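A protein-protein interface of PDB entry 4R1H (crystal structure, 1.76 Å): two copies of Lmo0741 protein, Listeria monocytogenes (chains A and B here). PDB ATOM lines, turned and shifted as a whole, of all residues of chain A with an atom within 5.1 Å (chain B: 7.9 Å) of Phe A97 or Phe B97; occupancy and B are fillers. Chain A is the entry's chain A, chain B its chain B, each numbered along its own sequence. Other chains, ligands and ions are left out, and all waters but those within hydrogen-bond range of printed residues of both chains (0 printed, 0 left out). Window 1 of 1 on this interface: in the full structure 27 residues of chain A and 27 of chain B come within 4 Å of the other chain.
Leu A93 touches Phe B97, and with the chains exchanged Phe A97 touches Leu B93.
Thr A94 touches Met B101, and with the chains exchanged Met A101 touches Thr B94.
Thr A94 touches Val B115, and with the chains exchanged Val A115 touches Thr B94.
Ile A98 touches Val B115, and with the chains exchanged Val A115 touches Ile B98.
13 positions are printed for both chains.
Of the printed residues of chain B, Leu A93 touches Phe B97 (3.7 Å), Glu B100 (3.96 Å), Met B101 (3.8 Å) and Leu B104 (3.97 Å).
Of chain B, only Leu B93 (3.7 Å), Thr B94 (3.6 Å) and Phe B97 (3.5 Å) come within 4 Å of Phe A97.
Of chain A, only Leu A93 (3.7 Å), Thr A94 (3.5 Å) and Phe A97 (3.5 Å) come within 4 Å of Phe B97.
Printed residues of chain A within 4 Å of Ile B111: Val A115 (3.9 Å).
Printed residues of chain A within 4 Å of Ile B112: Val A115.
The nearest residue of chain B that does not touch Phe A97 is Val B115 (4.4 Å).
The nearest printed residue of chain A that does not touch Val B115 is Ile A111 (4.05 Å).
Of the 23 printed residues of chain B, 12 touch a printed residue of chain A.
Printed residues of chain B that touch a printed residue of chain A: Leu B93, Thr B94, Phe B97, Ile B98, Glu B100, Met B101, Leu B104, Ile B111, Ile B112, Trp B114, Val B115 and Val B118.
Of the 13 printed residues of chain A, 8 touch a printed residue of chain B.
Among the printed residues, 22 pairs touch across the chains.
O of Ile A98 sits at hydrogen-bond distance from OG of Ser A102 (2.7 Å).
The backbone carbonyl oxygen (O) of Ala B90 is in hydrogen-bond range of the side-chain hydroxyl (OG1) of Thr B94, at 2.8 Å.
The backbone carbonyl oxygen (O) of Ile B98 is in hydrogen-bond range of the side-chain hydroxyl (OG) of Ser B102, 2.7 Å away.
The side-chain carboxylate (OE2) of Glu B100 lies within salt-bridge range of the side-chain amino group (NZ) of Lys B103.
The backbone NH of Ile B106 is in hydrogen-bond range of the backbone carbonyl oxygen of Met B101.
Leu A93 touches Phe B97.
Leu A93 touches Glu B100.
CG2 of Thr A94 touches O of Trp B114, 3.6 Å away.
Leu B93 touches Phe A97.
Phe A97 touches Thr B94 (CZ to OG1, 3.6 Å).
CD2 of Phe A97 touches CD2 of Phe B97, at 3.5 Å.
CD1 of Ile A98 touches O of Val B115, 3.8 Å away.
Val B118 touches Ile A98 (O to CD1, 3.5 Å).
Val A115 touches Ile B111.
Val A115 touches Ile B112 (CG1 to CG1, 3.9 Å).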
ATOM      1  N   GLN A  92      28.153  28.702 -21.062  1.00  0.00           N
ATOM      2  CA  GLN A  92      28.940  27.603 -21.544  1.00  0.00           C
ATOM      3  C   GLN A  92      28.142  26.291 -21.629  1.00  0.00           C
ATOM      4  O   GLN A  92      28.257  25.541 -22.618  1.00  0.00           O
ATOM      5  CB  GLN A  92      30.191  27.407 -20.717  1.00  0.00           C
ATOM      6  CG  GLN A  92      31.132  26.374 -21.328  1.00  0.00           C
ATOM      7  CD  GLN A  92      31.814  26.851 -22.593  1.00  0.00           C
ATOM      8  OE1 GLN A  92      32.723  27.693 -22.551  1.00  0.00           O
ATOM      9  NE2 GLN A  92      31.419  26.280 -23.734  1.00  0.00           N
ATOM     10  N   LEU A  93      27.347  26.020 -20.628  1.00  0.00           N
ATOM     11  CA  LEU A  93      26.511  24.865 -20.664  1.00  0.00           C
ATOM     12  C   LEU A  93      25.542  24.894 -21.839  1.00  0.00           C
ATOM     13  O   LEU A  93      25.371  23.868 -22.541  1.00  0.00           O
ATOM     14  CB  LEU A  93      25.709  24.695 -19.391  1.00  0.00           C
ATOM     15  CG  LEU A  93      26.449  24.274 -18.109  1.00  0.00           C
ATOM     16  CD1 LEU A  93      25.595  24.457 -16.863  1.00  0.00           C
ATOM     17  CD2 LEU A  93      26.908  22.860 -18.244  1.00  0.00           C
ATOM     18  N   THR A  94      24.932  26.020 -22.060  1.00  0.00           N
ATOM     19  CA  THR A  94      23.946  26.212 -23.125  1.00  0.00           C
ATOM     20  C   THR A  94      24.645  26.136 -24.511  1.00  0.00           C
ATOM     21  O   THR A  94      24.119  25.409 -25.403  1.00  0.00           O
ATOM     22  CB  THR A  94      23.196  27.486 -22.947  1.00  0.00           C
ATOM     23  OG1 THR A  94      22.602  27.513 -21.650  1.00  0.00           O
ATOM     24  CG2 THR A  94      22.088  27.594 -23.934  1.00  0.00           C
ATOM     25  N   GLU A  95      25.774  26.803 -24.694  1.00  0.00           N
ATOM     26  CA  GLU A  95      26.493  26.741 -25.978  1.00  0.00           C
ATOM     27  C   GLU A  95      26.870  25.285 -26.285  1.00  0.00           C
ATOM     28  O   GLU A  95      26.703  24.820 -27.448  1.00  0.00           O
ATOM     29  CB  GLU A  95      27.760  27.596 -25.957  1.00  0.00           C
ATOM     30  CG  GLU A  95      27.501  29.072 -26.017  1.00  0.00           C
ATOM     31  CD  GLU A  95      28.766  29.886 -25.710  1.00  0.00           C
ATOM     32  OE1 GLU A  95      29.758  29.347 -25.140  1.00  0.00           O
ATOM     33  OE2 GLU A  95      28.696  31.062 -26.054  1.00  0.00           O
ATOM     34  N   ASN A  96      27.375  24.556 -25.288  1.00  0.00           N
ATOM     35  CA  ASN A  96      27.775  23.181 -25.519  1.00  0.00           C
ATOM     36  C   ASN A  96      26.570  22.285 -25.918  1.00  0.00           C
ATOM     37  O   ASN A  96      26.716  21.435 -26.810  1.00  0.00           O
ATOM     38  CB  ASN A  96      28.465  22.599 -24.332  1.00  0.00           C
ATOM     39  CG  ASN A  96      29.867  23.208 -24.121  1.00  0.00           C
ATOM     40  OD1 ASN A  96      30.400  23.913 -24.970  1.00  0.00           O
ATOM     41  ND2 ASN A  96      30.423  22.921 -23.007  1.00  0.00           N
ATOM     42  N   PHE A  97      25.467  22.456 -25.220  1.00  0.00           N
ATOM     43  CA  PHE A  97      24.240  21.721 -25.492  1.00  0.00           C
ATOM     44  C   PHE A  97      23.727  22.011 -26.916  1.00  0.00           C
ATOM     45  O   PHE A  97      23.447  21.082 -27.676  1.00  0.00           O
ATOM     46  CB  PHE A  97      23.201  22.080 -24.445  1.00  0.00           C
ATOM     47  CG  PHE A  97      21.821  21.503 -24.686  1.00  0.00           C
ATOM     48  CD1 PHE A  97      21.630  20.141 -24.729  1.00  0.00           C
ATOM     49  CD2 PHE A  97      20.741  22.320 -24.860  1.00  0.00           C
ATOM     50  CE1 PHE A  97      20.372  19.643 -24.926  1.00  0.00           C
ATOM     51  CE2 PHE A  97      19.455  21.829 -25.109  1.00  0.00           C
ATOM     52  CZ  PHE A  97      19.287  20.464 -25.174  1.00  0.00           C
ATOM     53  N   ILE A  98      23.534  23.279 -27.205  1.00  0.00           N
ATOM     54  CA  ILE A  98      23.118  23.655 -28.555  1.00  0.00           C
ATOM     55  C   ILE A  98      24.081  23.072 -29.605  1.00  0.00           C
ATOM     56  O   ILE A  98      23.612  22.577 -30.669  1.00  0.00           O
ATOM     57  CB  ILE A  98      22.932  25.169 -28.665  1.00  0.00           C
ATOM     58  CG1 ILE A  98      21.728  25.574 -27.803  1.00  0.00           C
ATOM     59  CG2 ILE A  98      22.723  25.543 -30.149  1.00  0.00           C
ATOM     60  CD1 ILE A  98      21.668  27.043 -27.679  1.00  0.00           C
ATOM     61  N   SER A  99      25.400  23.162 -29.409  1.00  0.00           N
ATOM     62  CA  SER A  99      26.338  22.600 -30.369  1.00  0.00           C
ATOM     63  C   SER A  99      26.119  21.097 -30.598  1.00  0.00           C
ATOM     64  O   SER A  99      26.043  20.605 -31.751  1.00  0.00           O
ATOM     65  CB  SER A  99      27.758  22.894 -29.920  1.00  0.00           C
ATOM     66  OG  SER A  99      28.656  22.245 -30.763  1.00  0.00           O
ATOM     67  N   GLU A 100      26.001  20.352 -29.512  1.00  0.00           N
ATOM     68  CA  GLU A 100      25.862  18.906 -29.645  1.00  0.00           C
ATOM     69  C   GLU A 100      24.532  18.544 -30.330  1.00  0.00           C
ATOM     70  O   GLU A 100      24.503  17.641 -31.157  1.00  0.00           O
ATOM     71  CB  GLU A 100      25.925  18.246 -28.252  1.00  0.00           C
ATOM     72  CG  GLU A 100      27.299  18.202 -27.642  1.00  0.00           C
ATOM     73  CD  GLU A 100      28.400  17.630 -28.516  1.00  0.00           C
ATOM     74  OE1 GLU A 100      28.229  16.518 -29.101  1.00  0.00           O
ATOM     75  OE2 GLU A 100      29.472  18.283 -28.618  1.00  0.00           O
ATOM     76  N   MET A 101      23.477  19.217 -29.975  1.00  0.00           N
ATOM     77  CA  MET A 101      22.187  18.976 -30.612  1.00  0.00           C
ATOM     78  C   MET A 101      22.197  19.354 -32.096  1.00  0.00           C
ATOM     79  O   MET A 101      21.624  18.642 -32.928  1.00  0.00           O
ATOM     80  CB  MET A 101      21.056  19.644 -29.885  1.00  0.00           C
ATOM     81  CG  MET A 101      20.925  19.184 -28.432  1.00  0.00           C
ATOM     82  SD  MET A 101      19.943  17.511 -28.313  1.00  0.00           S
ATOM     83  CE  MET A 101      18.199  18.204 -28.388  1.00  0.00           C
ATOM     84  N   SER A 102      22.844  20.476 -32.383  1.00  0.00           N
ATOM     85  CA  SER A 102      22.942  21.006 -33.749  1.00  0.00           C
ATOM     86  C   SER A 102      23.684  20.017 -34.621  1.00  0.00           C
ATOM     87  O   SER A 102      23.286  19.818 -35.789  1.00  0.00           O
ATOM     88  CB  SER A 102      23.603  22.345 -33.752  1.00  0.00           C
ATOM     89  OG  SER A 102      22.745  23.297 -33.143  1.00  0.00           O
ATOM     90  N   ILE A 111      15.118  21.794 -30.575  1.00  0.00           N
ATOM     91  CA  ILE A 111      15.902  21.825 -29.311  1.00  0.00           C
ATOM     92  C   ILE A 111      15.050  22.376 -28.169  1.00  0.00           C
ATOM     93  O   ILE A 111      14.981  21.805 -27.071  1.00  0.00           O
ATOM     94  CB  ILE A 111      17.223  22.635 -29.439  1.00  0.00           C
ATOM     95  CG1 ILE A 111      18.136  21.989 -30.449  1.00  0.00           C
ATOM     96  CG2 ILE A 111      17.954  22.709 -28.061  1.00  0.00           C
ATOM     97  CD1 ILE A 111      19.362  22.797 -30.843  1.00  0.00           C
ATOM     98  N   VAL A 115      13.735  20.473 -24.656  1.00  0.00           N
ATOM     99  CA  VAL A 115      13.898  21.053 -23.313  1.00  0.00           C
ATOM    100  C   VAL A 115      12.567  21.118 -22.602  1.00  0.00           C
ATOM    101  O   VAL A 115      12.448  20.784 -21.403  1.00  0.00           O
ATOM    102  CB  VAL A 115      14.582  22.447 -23.399  1.00  0.00           C
ATOM    103  CG1 VAL A 115      14.496  23.126 -22.041  1.00  0.00           C
ATOM    104  CG2 VAL A 115      16.007  22.341 -23.877  1.00  0.00           C
ATOM    105  N   ILE B  89      19.658   9.586 -27.898  1.00  0.00           N
ATOM    106  CA  ILE B  89      20.771  10.500 -27.848  1.00  0.00           C
ATOM    107  C   ILE B  89      20.295  11.892 -27.397  1.00  0.00           C
ATOM    108  O   ILE B  89      20.935  12.520 -26.485  1.00  0.00           O
ATOM    109  CB  ILE B  89      21.530  10.609 -29.192  1.00  0.00           C
ATOM    110  CG1 ILE B  89      22.225   9.249 -29.496  1.00  0.00           C
ATOM    111  CG2 ILE B  89      22.569  11.657 -29.046  1.00  0.00           C
ATOM    112  CD1 ILE B  89      22.801   9.198 -30.838  1.00  0.00           C
ATOM    113  N   ALA B  90      19.236  12.378 -28.028  1.00  0.00           N
ATOM    114  CA  ALA B  90      18.711  13.750 -27.727  1.00  0.00           C
ATOM    115  C   ALA B  90      18.187  13.789 -26.288  1.00  0.00           C
ATOM    116  O   ALA B  90      18.402  14.775 -25.550  1.00  0.00           O
ATOM    117  CB  ALA B  90      17.637  14.146 -28.644  1.00  0.00           C
ATOM    118  N   LYS B  91      17.544  12.724 -25.848  1.00  0.00           N
ATOM    119  CA  LYS B  91      16.990  12.721 -24.502  1.00  0.00           C
ATOM    120  C   LYS B  91      18.114  12.790 -23.476  1.00  0.00           C
ATOM    121  O   LYS B  91      18.019  13.516 -22.491  1.00  0.00           O
ATOM    122  CB  LYS B  91      16.153  11.441 -24.292  1.00  0.00           C
ATOM    123  CG  LYS B  91      15.760  11.220 -22.817  1.00  0.00           C
ATOM    124  CD  LYS B  91      14.768  10.043 -22.768  1.00  0.00           C
ATOM    125  CE  LYS B  91      14.701   9.375 -21.407  1.00  0.00           C
ATOM    126  NZ  LYS B  91      14.271   7.965 -21.635  1.00  0.00           N
ATOM    127  N   GLN B  92      19.199  12.044 -23.672  1.00  0.00           N
ATOM    128  CA  GLN B  92      20.289  12.068 -22.739  1.00  0.00           C
ATOM    129  C   GLN B  92      21.005  13.383 -22.733  1.00  0.00           C
ATOM    130  O   GLN B  92      21.305  13.936 -21.629  1.00  0.00           O
ATOM    131  CB  GLN B  92      21.311  10.977 -23.058  1.00  0.00           C
ATOM    132  CG  GLN B  92      22.517  10.988 -22.167  1.00  0.00           C
ATOM    133  CD  GLN B  92      23.043   9.614 -21.956  1.00  0.00           C
ATOM    134  OE1 GLN B  92      23.521   8.994 -22.892  1.00  0.00           O
ATOM    135  NE2 GLN B  92      22.867   9.082 -20.742  1.00  0.00           N
ATOM    136  N   LEU B  93      21.221  13.991 -23.915  1.00  0.00           N
ATOM    137  CA  LEU B  93      21.870  15.295 -23.916  1.00  0.00           C
ATOM    138  C   LEU B  93      20.977  16.320 -23.129  1.00  0.00           C
ATOM    139  O   LEU B  93      21.473  17.173 -22.363  1.00  0.00           O
ATOM    140  CB  LEU B  93      22.006  15.827 -25.332  1.00  0.00           C
ATOM    141  CG  LEU B  93      23.216  15.161 -26.030  1.00  0.00           C
ATOM    142  CD1 LEU B  93      23.067  15.492 -27.525  1.00  0.00           C
ATOM    143  CD2 LEU B  93      24.500  15.829 -25.584  1.00  0.00           C
ATOM    144  N   THR B  94      19.698  16.244 -23.387  1.00  0.00           N
ATOM    145  CA  THR B  94      18.748  17.206 -22.789  1.00  0.00           C
ATOM    146  C   THR B  94      18.641  16.964 -21.280  1.00  0.00           C
ATOM    147  O   THR B  94      18.688  17.936 -20.493  1.00  0.00           O
ATOM    148  CB  THR B  94      17.391  17.107 -23.500  1.00  0.00           C
ATOM    149  OG1 THR B  94      17.538  17.372 -24.914  1.00  0.00           O
ATOM    150  CG2 THR B  94      16.409  18.138 -22.985  1.00  0.00           C
ATOM    151  N   GLU B  95      18.450  15.722 -20.865  1.00  0.00           N
ATOM    152  CA  GLU B  95      18.426  15.451 -19.419  1.00  0.00           C
ATOM    153  C   GLU B  95      19.673  15.962 -18.734  1.00  0.00           C
ATOM    154  O   GLU B  95      19.580  16.524 -17.619  1.00  0.00           O
ATOM    155  CB  GLU B  95      18.355  13.970 -19.150  1.00  0.00           C
ATOM    156  CG  GLU B  95      17.040  13.389 -19.411  1.00  0.00           C
ATOM    157  CD  GLU B  95      17.083  11.826 -19.355  1.00  0.00           C
ATOM    158  OE1 GLU B  95      18.151  11.118 -19.447  1.00  0.00           O
ATOM    159  OE2 GLU B  95      15.958  11.361 -19.372  1.00  0.00           O
ATOM    160  N   ASN B  96      20.851  15.667 -19.297  1.00  0.00           N
ATOM    161  CA  ASN B  96      22.075  16.115 -18.697  1.00  0.00           C
ATOM    162  C   ASN B  96      22.158  17.627 -18.592  1.00  0.00           C
ATOM    163  O   ASN B  96      22.559  18.140 -17.531  1.00  0.00           O
ATOM    164  CB  ASN B  96      23.283  15.559 -19.419  1.00  0.00           C
ATOM    165  CG  ASN B  96      23.433  14.051 -19.168  1.00  0.00           C
ATOM    166  OD1 ASN B  96      22.716  13.452 -18.326  1.00  0.00           O
ATOM    167  ND2 ASN B  96      24.264  13.433 -19.946  1.00  0.00           N
ATOM    168  N   PHE B  97      21.796  18.316 -19.663  1.00  0.00           N
ATOM    169  CA  PHE B  97      21.761  19.777 -19.658  1.00  0.00           C
ATOM    170  C   PHE B  97      20.841  20.334 -18.583  1.00  0.00           C
ATOM    171  O   PHE B  97      21.251  21.215 -17.800  1.00  0.00           O
ATOM    172  CB  PHE B  97      21.391  20.271 -21.044  1.00  0.00           C
ATOM    173  CG  PHE B  97      21.157  21.768 -21.162  1.00  0.00           C
ATOM    174  CD1 PHE B  97      22.192  22.684 -20.902  1.00  0.00           C
ATOM    175  CD2 PHE B  97      19.909  22.275 -21.477  1.00  0.00           C
ATOM    176  CE1 PHE B  97      22.017  24.037 -20.985  1.00  0.00           C
ATOM    177  CE2 PHE B  97      19.728  23.651 -21.598  1.00  0.00           C
ATOM    178  CZ  PHE B  97      20.772  24.535 -21.343  1.00  0.00           C
ATOM    179  N   ILE B  98      19.609  19.838 -18.554  1.00  0.00           N
ATOM    180  CA  ILE B  98      18.619  20.360 -17.556  1.00  0.00           C
ATOM    181  C   ILE B  98      19.161  20.055 -16.155  1.00  0.00           C
ATOM    182  O   ILE B  98      19.056  20.920 -15.267  1.00  0.00           O
ATOM    183  CB  ILE B  98      17.262  19.766 -17.782  1.00  0.00           C
ATOM    184  CG1 ILE B  98      16.650  20.331 -19.038  1.00  0.00           C
ATOM    185  CG2 ILE B  98      16.309  20.038 -16.575  1.00  0.00           C
ATOM    186  CD1 ILE B  98      15.435  19.591 -19.548  1.00  0.00           C
ATOM    187  N   SER B  99      19.776  18.897 -15.958  1.00  0.00           N
ATOM    188  CA  SER B  99      20.369  18.532 -14.669  1.00  0.00           C
ATOM    189  C   SER B  99      21.430  19.535 -14.257  1.00  0.00           C
ATOM    190  O   SER B  99      21.446  20.023 -13.118  1.00  0.00           O
ATOM    191  CB  SER B  99      21.005  17.116 -14.688  1.00  0.00           C
ATOM    192  OG  SER B  99      21.427  16.844 -13.381  1.00  0.00           O
ATOM    193  N   GLU B 100      22.340  19.853 -15.168  1.00  0.00           N
ATOM    194  CA  GLU B 100      23.393  20.739 -14.843  1.00  0.00           C
ATOM    195  C   GLU B 100      22.896  22.182 -14.555  1.00  0.00           C
ATOM    196  O   GLU B 100      23.454  22.864 -13.643  1.00  0.00           O
ATOM    197  CB  GLU B 100      24.452  20.786 -15.924  1.00  0.00           C
ATOM    198  CG  GLU B 100      25.236  19.504 -16.063  1.00  0.00           C
ATOM    199  CD  GLU B 100      25.969  19.095 -14.791  1.00  0.00           C
ATOM    200  OE1 GLU B 100      26.633  19.932 -14.180  1.00  0.00           O
ATOM    201  OE2 GLU B 100      25.814  17.943 -14.352  1.00  0.00           O
ATOM    202  N   MET B 101      21.942  22.645 -15.342  1.00  0.00           N
ATOM    203  CA  MET B 101      21.329  23.956 -15.150  1.00  0.00           C
ATOM    204  C   MET B 101      20.587  24.004 -13.814  1.00  0.00           C
ATOM    205  O   MET B 101      20.637  24.997 -13.080  1.00  0.00           O
ATOM    206  CB  MET B 101      20.421  24.337 -16.315  1.00  0.00           C
ATOM    207  CG  MET B 101      21.247  24.506 -17.588  1.00  0.00           C
ATOM    208  SD  MET B 101      22.283  26.100 -17.734  1.00  0.00           S
ATOM    209  CE  MET B 101      20.834  27.221 -18.410  1.00  0.00           C
ATOM    210  N   SER B 102      19.872  22.938 -13.495  1.00  0.00           N
ATOM    211  CA  SER B 102      19.074  22.829 -12.253  1.00  0.00           C
ATOM    212  C   SER B 102      19.987  22.877 -11.045  1.00  0.00           C
ATOM    213  O   SER B 102      19.643  23.411  -9.989  1.00  0.00           O
ATOM    214  CB  SER B 102      18.272  21.559 -12.240  1.00  0.00           C
ATOM    215  OG  SER B 102      17.286  21.631 -13.290  1.00  0.00           O
ATOM    216  N   LYS B 103      21.161  22.311 -11.156  1.00  0.00           N
ATOM    217  CA  LYS B 103      22.127  22.374 -10.048  1.00  0.00           C
ATOM    218  C   LYS B 103      22.594  23.752  -9.732  1.00  0.00           C
ATOM    219  O   LYS B 103      23.040  23.990  -8.628  1.00  0.00           O
ATOM    220  CB  LYS B 103      23.346  21.466 -10.292  1.00  0.00           C
ATOM    221  CG  LYS B 103      23.002  19.991 -10.219  1.00  0.00           C
ATOM    222  CD  LYS B 103      24.232  19.217 -10.684  1.00  0.00           C
ATOM    223  CE  LYS B 103      23.934  17.727 -10.732  1.00  0.00           C
ATOM    224  NZ  LYS B 103      25.043  17.044 -11.462  1.00  0.00           N
ATOM    225  N   LEU B 104      22.502  24.682 -10.670  1.00  0.00           N
ATOM    226  CA  LEU B 104      22.837  26.075 -10.463  1.00  0.00           C
ATOM    227  C   LEU B 104      21.595  26.893  -9.980  1.00  0.00           C
ATOM    228  O   LEU B 104      21.675  28.116  -9.855  1.00  0.00           O
ATOM    229  CB  LEU B 104      23.253  26.680 -11.769  1.00  0.00           C
ATOM    230  CG  LEU B 104      24.458  26.037 -12.420  1.00  0.00           C
ATOM    231  CD1 LEU B 104      24.674  26.735 -13.742  1.00  0.00           C
ATOM    232  CD2 LEU B 104      25.613  26.203 -11.472  1.00  0.00           C
ATOM    233  N   ILE B 106      18.674  27.173 -11.723  1.00  0.00           N
ATOM    234  CA  ILE B 106      18.014  27.865 -12.811  1.00  0.00           C
ATOM    235  C   ILE B 106      16.780  27.054 -13.155  1.00  0.00           C
ATOM    236  O   ILE B 106      16.840  25.859 -13.469  1.00  0.00           O
ATOM    237  CB  ILE B 106      18.949  27.973 -14.029  1.00  0.00           C
ATOM    238  CG1 ILE B 106      20.188  28.749 -13.622  1.00  0.00           C
ATOM    239  CG2 ILE B 106      18.238  28.641 -15.166  1.00  0.00           C
ATOM    240  CD1 ILE B 106      21.164  28.931 -14.720  1.00  0.00           C
ATOM    241  N   LYS B 110      13.734  29.763 -17.193  1.00  0.00           N
ATOM    242  CA  LYS B 110      15.004  30.461 -17.423  1.00  0.00           C
ATOM    243  C   LYS B 110      15.991  29.596 -18.289  1.00  0.00           C
ATOM    244  O   LYS B 110      16.754  30.133 -19.063  1.00  0.00           O
ATOM    245  CB  LYS B 110      15.664  30.900 -16.142  1.00  0.00           C
ATOM    246  CG  LYS B 110      16.753  31.916 -16.367  1.00  0.00           C
ATOM    247  CD  LYS B 110      17.021  32.716 -15.100  1.00  0.00           C
ATOM    248  CE  LYS B 110      18.098  33.746 -15.280  1.00  0.00           C
ATOM    249  NZ  LYS B 110      17.999  34.655 -14.068  1.00  0.00           N
ATOM    250  N   ILE B 111      15.863  28.305 -18.144  1.00  0.00           N
ATOM    251  CA  ILE B 111      16.588  27.365 -19.025  1.00  0.00           C
ATOM    252  C   ILE B 111      16.160  27.610 -20.470  1.00  0.00           C
ATOM    253  O   ILE B 111      17.017  27.724 -21.366  1.00  0.00           O
ATOM    254  CB  ILE B 111      16.427  25.911 -18.633  1.00  0.00           C
ATOM    255  CG1 ILE B 111      17.115  25.642 -17.296  1.00  0.00           C
ATOM    256  CG2 ILE B 111      17.018  24.983 -19.704  1.00  0.00           C
ATOM    257  CD1 ILE B 111      16.851  24.304 -16.664  1.00  0.00           C
ATOM    258  N   ILE B 112      14.874  27.638 -20.701  1.00  0.00           N
ATOM    259  CA  ILE B 112      14.320  27.902 -22.021  1.00  0.00           C
ATOM    260  C   ILE B 112      14.794  29.247 -22.534  1.00  0.00           C
ATOM    261  O   ILE B 112      15.163  29.414 -23.715  1.00  0.00           O
ATOM    262  CB  ILE B 112      12.767  27.833 -22.004  1.00  0.00           C
ATOM    263  CG1 ILE B 112      12.371  26.372 -21.738  1.00  0.00           C
ATOM    264  CG2 ILE B 112      12.212  28.291 -23.335  1.00  0.00           C
ATOM    265  CD1 ILE B 112      10.983  26.174 -21.233  1.00  0.00           C
ATOM    266  N   TRP B 114      17.601  30.814 -21.777  1.00  0.00           N
ATOM    267  CA  TRP B 114      19.000  30.618 -22.185  1.00  0.00           C
ATOM    268  C   TRP B 114      19.092  29.963 -23.616  1.00  0.00           C
ATOM    269  O   TRP B 114      19.864  30.385 -24.441  1.00  0.00           O
ATOM    270  CB  TRP B 114      19.732  29.747 -21.158  1.00  0.00           C
ATOM    271  CG  TRP B 114      20.367  30.614 -20.138  1.00  0.00           C
ATOM    272  CD1 TRP B 114      19.947  30.820 -18.833  1.00  0.00           C
ATOM    273  CD2 TRP B 114      21.532  31.355 -20.294  1.00  0.00           C
ATOM    274  NE1 TRP B 114      20.791  31.717 -18.196  1.00  0.00           N
ATOM    275  CE2 TRP B 114      21.762  32.071 -19.068  1.00  0.00           C
ATOM    276  CE3 TRP B 114      22.403  31.564 -21.345  1.00  0.00           C
ATOM    277  CZ2 TRP B 114      22.810  32.930 -18.911  1.00  0.00           C
ATOM    278  CZ3 TRP B 114      23.418  32.445 -21.176  1.00  0.00           C
ATOM    279  CH2 TRP B 114      23.620  33.114 -19.970  1.00  0.00           C
ATOM    280  N   VAL B 115      18.307  28.912 -23.814  1.00  0.00           N
ATOM    281  CA  VAL B 115      18.376  28.176 -25.099  1.00  0.00           C
ATOM    282  C   VAL B 115      17.929  29.078 -26.230  1.00  0.00           C
ATOM    283  O   VAL B 115      18.539  29.082 -27.327  1.00  0.00           O
ATOM    284  CB  VAL B 115      17.536  26.916 -25.018  1.00  0.00           C
ATOM    285  CG1 VAL B 115      17.411  26.359 -26.398  1.00  0.00           C
ATOM    286  CG2 VAL B 115      18.078  25.913 -24.016  1.00  0.00           C
ATOM    287  N   VAL B 118      20.864  31.886 -26.874  1.00  0.00           N
ATOM    288  CA  VAL B 118      22.166  31.498 -27.384  1.00  0.00           C
ATOM    289  C   VAL B 118      22.138  31.041 -28.871  1.00  0.00           C
ATOM    290  O   VAL B 118      21.393  30.158 -29.256  1.00  0.00           O
ATOM    291  CB  VAL B 118      22.773  30.433 -26.461  1.00  0.00           C
ATOM    292  CG1 VAL B 118      23.989  29.757 -27.054  1.00  0.00           C
ATOM    293  CG2 VAL B 118      23.081  31.080 -25.099  1.00  0.00           C
